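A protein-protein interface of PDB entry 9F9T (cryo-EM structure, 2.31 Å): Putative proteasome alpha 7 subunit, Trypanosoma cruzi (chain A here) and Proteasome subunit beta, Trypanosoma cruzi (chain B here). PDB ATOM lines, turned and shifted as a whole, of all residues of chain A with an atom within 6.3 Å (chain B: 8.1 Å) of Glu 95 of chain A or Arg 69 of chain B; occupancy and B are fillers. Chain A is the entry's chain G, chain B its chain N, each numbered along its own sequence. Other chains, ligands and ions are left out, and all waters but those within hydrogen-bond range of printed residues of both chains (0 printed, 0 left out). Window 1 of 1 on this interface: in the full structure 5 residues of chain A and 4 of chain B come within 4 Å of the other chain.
ND2 of Asn 65 of chain B sits at hydrogen-bond distance from OD1 of Asp 99 of chain A (3.2 Å). The guanidinium group of Arg 69 of chain B is in salt-bridge range of the side-chain carboxylate of Glu 95 of chain A, at 3.8 Å. NH2 of Arg 69 of chain B lies within salt-bridge range of OD2 of Asp 99 of chain A, at 2.8 Å. The side-chain carboxylate (OE1) of Glu 95 of chain A lies within hydrogen-bond range of the side-chain hydroxyl (OH) of Tyr 73 of chain B, at 2.6 Å.
The backbone carbonyl oxygen (O) of Thr 61 of chain B lies close to the side-chain amide nitrogen (ND2) of Asn 65 of chain B (3.4 Å). NE of Arg 98 of chain A is in salt-bridge range of OD1 of Asp 69 of chain A (2.9 Å).
Asp 69 of chain A touches Met 72 of chain B (C to SD, 3.7 Å). Tyr 73 of chain B touches Arg 91 of chain A (CE1 to CD, 3.5 Å).
Glu 95 of chain A touches just these residues of chain B: Arg 69 and Tyr 73. Arg 69 of chain B touches just these residues of chain A: Glu 95 (3.4 Å) and Asp 99 (2.8 Å). No residue of chain B comes within 4 Å of Ala 94 of chain A. Printed residues of chain A within 4 Å of Asn 65 of chain B: Asp 99. Of the printed residues of chain B, Asp 69 of chain A touches Met 72. Thr 61 of chain B touches none of the printed residues of chain A. The nearest residue of chain B that does not touch Glu 95 of chain A is Asn 65 of chain B (6.3 Å).
Printed residues of chain A that touch a printed residue of chain B: Asp 69, Arg 91, Glu 95 and Asp 99. Of the 16 printed residues of chain B, 4 touch a printed residue of chain A. Among the printed residues, 6 pairs touch across the chains.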
ATOM      1  N   VAL A  68     -24.128  29.945  22.880  1.00  0.00           N
ATOM      2  CA  VAL A  68     -24.211  29.965  21.433  1.00  0.00           C
ATOM      3  C   VAL A  68     -23.888  28.635  20.828  1.00  0.00           C
ATOM      4  O   VAL A  68     -24.221  28.399  19.674  1.00  0.00           O
ATOM      5  CB  VAL A  68     -23.431  31.113  20.794  1.00  0.00           C
ATOM      6  CG1 VAL A  68     -24.099  32.419  21.176  1.00  0.00           C
ATOM      7  CG2 VAL A  68     -21.965  31.155  21.150  1.00  0.00           C
ATOM      8  N   ASP A  69     -23.222  27.794  21.623  1.00  0.00           N
ATOM      9  CA  ASP A  69     -22.760  26.473  21.203  1.00  0.00           C
ATOM     10  C   ASP A  69     -22.425  25.726  22.488  1.00  0.00           C
ATOM     11  O   ASP A  69     -22.532  26.237  23.589  1.00  0.00           O
ATOM     12  CB  ASP A  69     -21.528  26.565  20.318  1.00  0.00           C
ATOM     13  CG  ASP A  69     -21.157  25.298  19.512  1.00  0.00           C
ATOM     14  OD1 ASP A  69     -21.998  24.252  19.477  1.00  0.00           O
ATOM     15  OD2 ASP A  69     -20.007  25.323  18.886  1.00  0.00           O
ATOM     16  N   SER A  88     -28.561  35.305  17.695  1.00  0.00           N
ATOM     17  CA  SER A  88     -29.024  34.319  16.743  1.00  0.00           C
ATOM     18  C   SER A  88     -28.020  34.109  15.603  1.00  0.00           C
ATOM     19  O   SER A  88     -27.909  33.029  15.003  1.00  0.00           O
ATOM     20  CB  SER A  88     -30.344  34.678  16.216  1.00  0.00           C
ATOM     21  OG  SER A  88     -31.094  35.380  17.196  1.00  0.00           O
ATOM     22  N   ALA A  90     -24.701  34.498  15.936  1.00  0.00           N
ATOM     23  CA  ALA A  90     -23.659  33.722  16.533  1.00  0.00           C
ATOM     24  C   ALA A  90     -23.985  32.228  16.583  1.00  0.00           C
ATOM     25  O   ALA A  90     -23.075  31.409  16.445  1.00  0.00           O
ATOM     26  CB  ALA A  90     -23.362  34.242  17.899  1.00  0.00           C
ATOM     27  N   ARG A  91     -25.247  31.852  16.783  1.00  0.00           N
ATOM     28  CA  ARG A  91     -25.596  30.450  16.818  1.00  0.00           C
ATOM     29  C   ARG A  91     -25.553  29.875  15.409  1.00  0.00           C
ATOM     30  O   ARG A  91     -25.050  28.792  15.187  1.00  0.00           O
ATOM     31  CB  ARG A  91     -27.008  30.263  17.396  1.00  0.00           C
ATOM     32  CG  ARG A  91     -27.058  30.477  18.908  1.00  0.00           C
ATOM     33  CD  ARG A  91     -28.435  30.476  19.494  1.00  0.00           C
ATOM     34  NE  ARG A  91     -28.362  30.710  20.931  1.00  0.00           N
ATOM     35  CZ  ARG A  91     -29.421  30.753  21.714  1.00  0.00           C
ATOM     36  NH1 ARG A  91     -30.579  30.936  21.150  1.00  0.00           N
ATOM     37  NH2 ARG A  91     -29.322  30.738  23.018  1.00  0.00           N
ATOM     38  N   ALA A  92     -26.024  30.623  14.419  1.00  0.00           N
ATOM     39  CA  ALA A  92     -25.975  30.151  13.036  1.00  0.00           C
ATOM     40  C   ALA A  92     -24.526  29.898  12.609  1.00  0.00           C
ATOM     41  O   ALA A  92     -24.224  28.970  11.882  1.00  0.00           O
ATOM     42  CB  ALA A  92     -26.680  31.187  12.187  1.00  0.00           C
ATOM     43  N   GLU A  93     -23.628  30.772  13.034  1.00  0.00           N
ATOM     44  CA  GLU A  93     -22.235  30.613  12.728  1.00  0.00           C
ATOM     45  C   GLU A  93     -21.738  29.355  13.400  1.00  0.00           C
ATOM     46  O   GLU A  93     -21.085  28.529  12.751  1.00  0.00           O
ATOM     47  CB  GLU A  93     -21.358  31.762  13.240  1.00  0.00           C
ATOM     48  CG  GLU A  93     -21.693  33.111  12.610  1.00  0.00           C
ATOM     49  CD  GLU A  93     -21.455  33.356  11.118  1.00  0.00           C
ATOM     50  OE1 GLU A  93     -20.280  33.409  10.720  1.00  0.00           O
ATOM     51  OE2 GLU A  93     -22.443  33.546  10.360  1.00  0.00           O
ATOM     52  N   ALA A  94     -22.046  29.209  14.687  1.00  0.00           N
ATOM     53  CA  ALA A  94     -21.547  28.048  15.408  1.00  0.00           C
ATOM     54  C   ALA A  94     -22.080  26.768  14.773  1.00  0.00           C
ATOM     55  O   ALA A  94     -21.402  25.798  14.737  1.00  0.00           O
ATOM     56  CB  ALA A  94     -21.892  28.137  16.871  1.00  0.00           C
ATOM     57  N   GLU A  95     -23.280  26.814  14.226  1.00  0.00           N
ATOM     58  CA  GLU A  95     -23.942  25.630  13.682  1.00  0.00           C
ATOM     59  C   GLU A  95     -23.335  25.266  12.336  1.00  0.00           C
ATOM     60  O   GLU A  95     -22.999  24.103  12.097  1.00  0.00           O
ATOM     61  CB  GLU A  95     -25.413  25.893  13.441  1.00  0.00           C
ATOM     62  CG  GLU A  95     -26.238  25.847  14.700  1.00  0.00           C
ATOM     63  CD  GLU A  95     -27.573  26.610  14.503  1.00  0.00           C
ATOM     64  OE1 GLU A  95     -28.287  26.925  15.556  1.00  0.00           O
ATOM     65  OE2 GLU A  95     -27.926  26.912  13.299  1.00  0.00           O
ATOM     66  N   ASN A  96     -23.169  26.329  11.537  1.00  0.00           N
ATOM     67  CA  ASN A  96     -22.423  26.317  10.300  1.00  0.00           C
ATOM     68  C   ASN A  96     -21.096  25.599  10.470  1.00  0.00           C
ATOM     69  O   ASN A  96     -20.785  24.709   9.702  1.00  0.00           O
ATOM     70  CB  ASN A  96     -22.127  27.726   9.776  1.00  0.00           C
ATOM     71  CG  ASN A  96     -21.562  27.697   8.369  1.00  0.00           C
ATOM     72  OD1 ASN A  96     -20.415  28.078   8.133  1.00  0.00           O
ATOM     73  ND2 ASN A  96     -22.343  27.146   7.461  1.00  0.00           N
ATOM     74  N   SER A  97     -20.302  26.007  11.423  1.00  0.00           N
ATOM     75  CA  SER A  97     -19.015  25.352  11.569  1.00  0.00           C
ATOM     76  C   SER A  97     -19.158  23.888  11.833  1.00  0.00           C
ATOM     77  O   SER A  97     -18.388  23.186  11.238  1.00  0.00           O
ATOM     78  CB  SER A  97     -18.163  25.919  12.593  1.00  0.00           C
ATOM     79  OG  SER A  97     -17.095  25.048  12.826  1.00  0.00           O
ATOM     80  N   ARG A  98     -20.116  23.419  12.625  1.00  0.00           N
ATOM     81  CA  ARG A  98     -20.285  21.968  12.830  1.00  0.00           C
ATOM     82  C   ARG A  98     -20.858  21.315  11.591  1.00  0.00           C
ATOM     83  O   ARG A  98     -20.356  20.284  11.193  1.00  0.00           O
ATOM     84  CB  ARG A  98     -21.186  21.655  14.033  1.00  0.00           C
ATOM     85  CG  ARG A  98     -20.583  22.227  15.307  1.00  0.00           C
ATOM     86  CD  ARG A  98     -21.334  21.990  16.579  1.00  0.00           C
ATOM     87  NE  ARG A  98     -20.534  22.359  17.755  1.00  0.00           N
ATOM     88  CZ  ARG A  98     -19.957  21.507  18.573  1.00  0.00           C
ATOM     89  NH1 ARG A  98     -19.870  20.253  18.201  1.00  0.00           N
ATOM     90  NH2 ARG A  98     -19.365  21.919  19.692  1.00  0.00           N
ATOM     91  N   ASP A  99     -21.818  21.951  10.931  1.00  0.00           N
ATOM     92  CA  ASP A  99     -22.424  21.350   9.765  1.00  0.00           C
ATOM     93  C   ASP A  99     -21.433  21.239   8.611  1.00  0.00           C
ATOM     94  O   ASP A  99     -21.242  20.169   8.047  1.00  0.00           O
ATOM     95  CB  ASP A  99     -23.724  22.066   9.392  1.00  0.00           C
ATOM     96  CG  ASP A  99     -24.762  21.835  10.508  1.00  0.00           C
ATOM     97  OD1 ASP A  99     -24.432  20.971  11.425  1.00  0.00           O
ATOM     98  OD2 ASP A  99     -25.869  22.499  10.510  1.00  0.00           O
ATOM     99  N   VAL A 100     -20.784  22.341   8.284  1.00  0.00           N
ATOM    100  CA  VAL A 100     -20.042  22.392   7.049  1.00  0.00           C
ATOM    101  C   VAL A 100     -18.618  21.913   7.260  1.00  0.00           C
ATOM    102  O   VAL A 100     -18.121  21.245   6.375  1.00  0.00           O
ATOM    103  CB  VAL A 100     -20.075  23.807   6.444  1.00  0.00           C
ATOM    104  CG1 VAL A 100     -19.055  23.865   5.334  1.00  0.00           C
ATOM    105  CG2 VAL A 100     -21.464  24.181   5.920  1.00  0.00           C
ATOM    106  N   THR B  61     -28.274  13.005  11.229  1.00  0.00           N
ATOM    107  CA  THR B  61     -27.506  14.174  11.555  1.00  0.00           C
ATOM    108  C   THR B  61     -28.450  15.355  11.776  1.00  0.00           C
ATOM    109  O   THR B  61     -28.365  16.059  12.781  1.00  0.00           O
ATOM    110  CB  THR B  61     -26.452  14.428  10.478  1.00  0.00           C
ATOM    111  OG1 THR B  61     -25.395  13.518  10.652  1.00  0.00           O
ATOM    112  CG2 THR B  61     -25.773  15.766  10.633  1.00  0.00           C
ATOM    113  N   MET B  62     -29.278  15.584  10.787  1.00  0.00           N
ATOM    114  CA  MET B  62     -30.322  16.558  10.822  1.00  0.00           C
ATOM    115  C   MET B  62     -31.162  16.442  12.098  1.00  0.00           C
ATOM    116  O   MET B  62     -31.237  17.378  12.880  1.00  0.00           O
ATOM    117  CB  MET B  62     -31.096  16.310   9.555  1.00  0.00           C
ATOM    118  CG  MET B  62     -32.123  17.299   9.225  1.00  0.00           C
ATOM    119  SD  MET B  62     -33.517  16.909  10.294  1.00  0.00           S
ATOM    120  CE  MET B  62     -34.540  15.946   9.176  1.00  0.00           C
ATOM    121  N   ILE B  63     -31.575  15.255  12.480  1.00  0.00           N
ATOM    122  CA  ILE B  63     -32.326  15.084  13.697  1.00  0.00           C
ATOM    123  C   ILE B  63     -31.525  15.355  14.938  1.00  0.00           C
ATOM    124  O   ILE B  63     -32.074  15.946  15.834  1.00  0.00           O
ATOM    125  CB  ILE B  63     -32.957  13.678  13.739  1.00  0.00           C
ATOM    126  CG1 ILE B  63     -34.036  13.572  12.691  1.00  0.00           C
ATOM    127  CG2 ILE B  63     -33.574  13.353  15.072  1.00  0.00           C
ATOM    128  CD1 ILE B  63     -34.499  12.163  12.530  1.00  0.00           C
ATOM    129  N   GLU B  64     -30.321  14.795  15.064  1.00  0.00           N
ATOM    130  CA  GLU B  64     -29.533  14.984  16.269  1.00  0.00           C
ATOM    131  C   GLU B  64     -29.268  16.462  16.425  1.00  0.00           C
ATOM    132  O   GLU B  64     -29.179  16.940  17.538  1.00  0.00           O
ATOM    133  CB  GLU B  64     -28.119  14.385  16.306  1.00  0.00           C
ATOM    134  CG  GLU B  64     -27.971  12.844  16.485  1.00  0.00           C
ATOM    135  CD  GLU B  64     -26.635  12.167  16.028  1.00  0.00           C
ATOM    136  OE1 GLU B  64     -26.652  10.964  15.546  1.00  0.00           O
ATOM    137  OE2 GLU B  64     -25.540  12.837  16.142  1.00  0.00           O
ATOM    138  N   ASN B  65     -29.064  17.172  15.336  1.00  0.00           N
ATOM    139  CA  ASN B  65     -28.832  18.585  15.485  1.00  0.00           C
ATOM    140  C   ASN B  65     -30.051  19.376  15.998  1.00  0.00           C
ATOM    141  O   ASN B  65     -29.897  20.273  16.808  1.00  0.00           O
ATOM    142  CB  ASN B  65     -28.400  19.226  14.163  1.00  0.00           C
ATOM    143  CG  ASN B  65     -26.990  18.878  13.758  1.00  0.00           C
ATOM    144  OD1 ASN B  65     -26.173  18.453  14.574  1.00  0.00           O
ATOM    145  ND2 ASN B  65     -26.730  19.016  12.468  1.00  0.00           N
ATOM    146  N   HIS B  66     -31.240  19.172  15.475  1.00  0.00           N
ATOM    147  CA  HIS B  66     -32.468  19.759  16.003  1.00  0.00           C
ATOM    148  C   HIS B  66     -32.588  19.431  17.476  1.00  0.00           C
ATOM    149  O   HIS B  66     -32.534  20.292  18.316  1.00  0.00           O
ATOM    150  CB  HIS B  66     -33.610  19.320  15.075  1.00  0.00           C
ATOM    151  CG  HIS B  66     -34.915  19.763  15.579  1.00  0.00           C
ATOM    152  ND1 HIS B  66     -35.328  21.067  15.599  1.00  0.00           N
ATOM    153  CD2 HIS B  66     -35.896  19.063  16.200  1.00  0.00           C
ATOM    154  CE1 HIS B  66     -36.508  21.113  16.200  1.00  0.00           C
ATOM    155  NE2 HIS B  66     -36.880  19.926  16.609  1.00  0.00           N
ATOM    156  N   VAL B  67     -32.479  18.191  17.849  1.00  0.00           N
ATOM    157  CA  VAL B  67     -32.577  17.809  19.247  1.00  0.00           C
ATOM    158  C   VAL B  67     -31.537  18.480  20.137  1.00  0.00           C
ATOM    159  O   VAL B  67     -31.868  18.924  21.209  1.00  0.00           O
ATOM    160  CB  VAL B  67     -32.508  16.277  19.391  1.00  0.00           C
ATOM    161  CG1 VAL B  67     -32.396  15.836  20.841  1.00  0.00           C
ATOM    162  CG2 VAL B  67     -33.669  15.563  18.713  1.00  0.00           C
ATOM    163  N   ASN B  68     -30.261  18.499  19.773  1.00  0.00           N
ATOM    164  CA  ASN B  68     -29.272  19.147  20.615  1.00  0.00           C
ATOM    165  C   ASN B  68     -29.424  20.675  20.653  1.00  0.00           C
ATOM    166  O   ASN B  68     -29.170  21.310  21.685  1.00  0.00           O
ATOM    167  CB  ASN B  68     -27.852  18.863  20.156  1.00  0.00           C
ATOM    168  CG  ASN B  68     -27.446  17.403  20.250  1.00  0.00           C
ATOM    169  OD1 ASN B  68     -27.967  16.646  21.070  1.00  0.00           O
ATOM    170  ND2 ASN B  68     -26.496  16.999  19.415  1.00  0.00           N
ATOM    171  N   ARG B  69     -29.847  21.272  19.525  1.00  0.00           N
ATOM    172  CA  ARG B  69     -29.926  22.716  19.503  1.00  0.00           C
ATOM    173  C   ARG B  69     -31.109  23.186  20.332  1.00  0.00           C
ATOM    174  O   ARG B  69     -31.008  24.156  21.090  1.00  0.00           O
ATOM    175  CB  ARG B  69     -30.018  23.283  18.083  1.00  0.00           C
ATOM    176  CG  ARG B  69     -28.653  23.268  17.396  1.00  0.00           C
ATOM    177  CD  ARG B  69     -28.800  23.278  15.903  1.00  0.00           C
ATOM    178  NE  ARG B  69     -27.645  22.818  15.188  1.00  0.00           N
ATOM    179  CZ  ARG B  69     -27.626  22.809  13.855  1.00  0.00           C
ATOM    180  NH1 ARG B  69     -28.696  23.214  13.192  1.00  0.00           N
ATOM    181  NH2 ARG B  69     -26.535  22.447  13.197  1.00  0.00           N
ATOM    182  N   GLN B  70     -32.229  22.482  20.185  1.00  0.00           N
ATOM    183  CA  GLN B  70     -33.424  22.813  20.929  1.00  0.00           C
ATOM    184  C   GLN B  70     -33.165  22.796  22.417  1.00  0.00           C
ATOM    185  O   GLN B  70     -33.638  23.645  23.108  1.00  0.00           O
ATOM    186  CB  GLN B  70     -34.543  21.844  20.525  1.00  0.00           C
ATOM    187  CG  GLN B  70     -35.842  22.128  21.268  1.00  0.00           C
ATOM    188  CD  GLN B  70     -37.120  22.147  20.468  1.00  0.00           C
ATOM    189  OE1 GLN B  70     -37.194  22.784  19.396  1.00  0.00           O
ATOM    190  NE2 GLN B  70     -38.129  21.561  21.100  1.00  0.00           N
ATOM    191  N   GLN B  71     -32.420  21.852  22.901  1.00  0.00           N
ATOM    192  CA  GLN B  71     -32.078  21.697  24.305  1.00  0.00           C
ATOM    193  C   GLN B  71     -31.158  22.814  24.825  1.00  0.00           C
ATOM    194  O   GLN B  71     -31.293  23.262  25.957  1.00  0.00           O
ATOM    195  CB  GLN B  71     -31.431  20.324  24.466  1.00  0.00           C
ATOM    196  CG  GLN B  71     -31.366  19.797  25.892  1.00  0.00           C
ATOM    197  CD  GLN B  71     -30.203  20.321  26.686  1.00  0.00           C
ATOM    198  OE1 GLN B  71     -29.059  20.297  26.243  1.00  0.00           O
ATOM    199  NE2 GLN B  71     -30.488  20.816  27.875  1.00  0.00           N
ATOM    200  N   MET B  72     -30.237  23.274  24.002  1.00  0.00           N
ATOM    201  CA  MET B  72     -29.156  24.202  24.340  1.00  0.00           C
ATOM    202  C   MET B  72     -29.678  25.648  24.325  1.00  0.00           C
ATOM    203  O   MET B  72     -29.206  26.510  25.094  1.00  0.00           O
ATOM    204  CB  MET B  72     -28.096  23.901  23.264  1.00  0.00           C
ATOM    205  CG  MET B  72     -26.876  24.787  23.058  1.00  0.00           C
ATOM    206  SD  MET B  72     -25.513  23.701  22.338  1.00  0.00           S
ATOM    207  CE  MET B  72     -26.027  23.502  20.626  1.00  0.00           C
ATOM    208  N   TYR B  73     -30.694  25.894  23.469  1.00  0.00           N
ATOM    209  CA  TYR B  73     -31.347  27.198  23.361  1.00  0.00           C
ATOM    210  C   TYR B  73     -32.685  27.286  24.126  1.00  0.00           C
ATOM    211  O   TYR B  73     -33.637  27.877  23.622  1.00  0.00           O
ATOM    212  CB  TYR B  73     -31.711  27.407  21.890  1.00  0.00           C
ATOM    213  CG  TYR B  73     -30.560  27.263  20.918  1.00  0.00           C
ATOM    214  CD1 TYR B  73     -29.213  27.261  21.306  1.00  0.00           C
ATOM    215  CD2 TYR B  73     -30.840  27.127  19.581  1.00  0.00           C
ATOM    216  CE1 TYR B  73     -28.190  27.093  20.385  1.00  0.00           C
ATOM    217  CE2 TYR B  73     -29.824  26.954  18.658  1.00  0.00           C
ATOM    218  CZ  TYR B  73     -28.504  26.913  19.057  1.00  0.00           C
ATOM    219  OH  TYR B  73     -27.593  26.742  18.033  1.00  0.00           O
ATOM    220  N   GLY B  74     -32.842  26.537  25.229  1.00  0.00           N
ATOM    221  CA  GLY B  74     -33.919  26.783  26.174  1.00  0.00           C
ATOM    222  C   GLY B  74     -35.239  26.067  25.912  1.00  0.00           C
ATOM    223  O   GLY B  74     -36.116  26.166  26.749  1.00  0.00           O
ATOM    224  N   GLY B  75     -35.346  25.261  24.864  1.00  0.00           N
ATOM    225  CA  GLY B  75     -36.580  24.552  24.531  1.00  0.00           C
ATOM    226  C   GLY B  75     -36.661  23.099  25.027  1.00  0.00           C
ATOM    227  O   GLY B  75     -37.524  22.338  24.586  1.00  0.00           O
ATOM    228  N   GLY B  76     -35.848  22.712  26.016  1.00  0.00           N
ATOM    229  CA  GLY B  76     -36.012  21.416  26.680  1.00  0.00           C
ATOM    230  C   GLY B  76     -35.551  20.237  25.818  1.00  0.00           C
ATOM    231  O   GLY B  76     -35.051  20.422  24.728  1.00  0.00           O
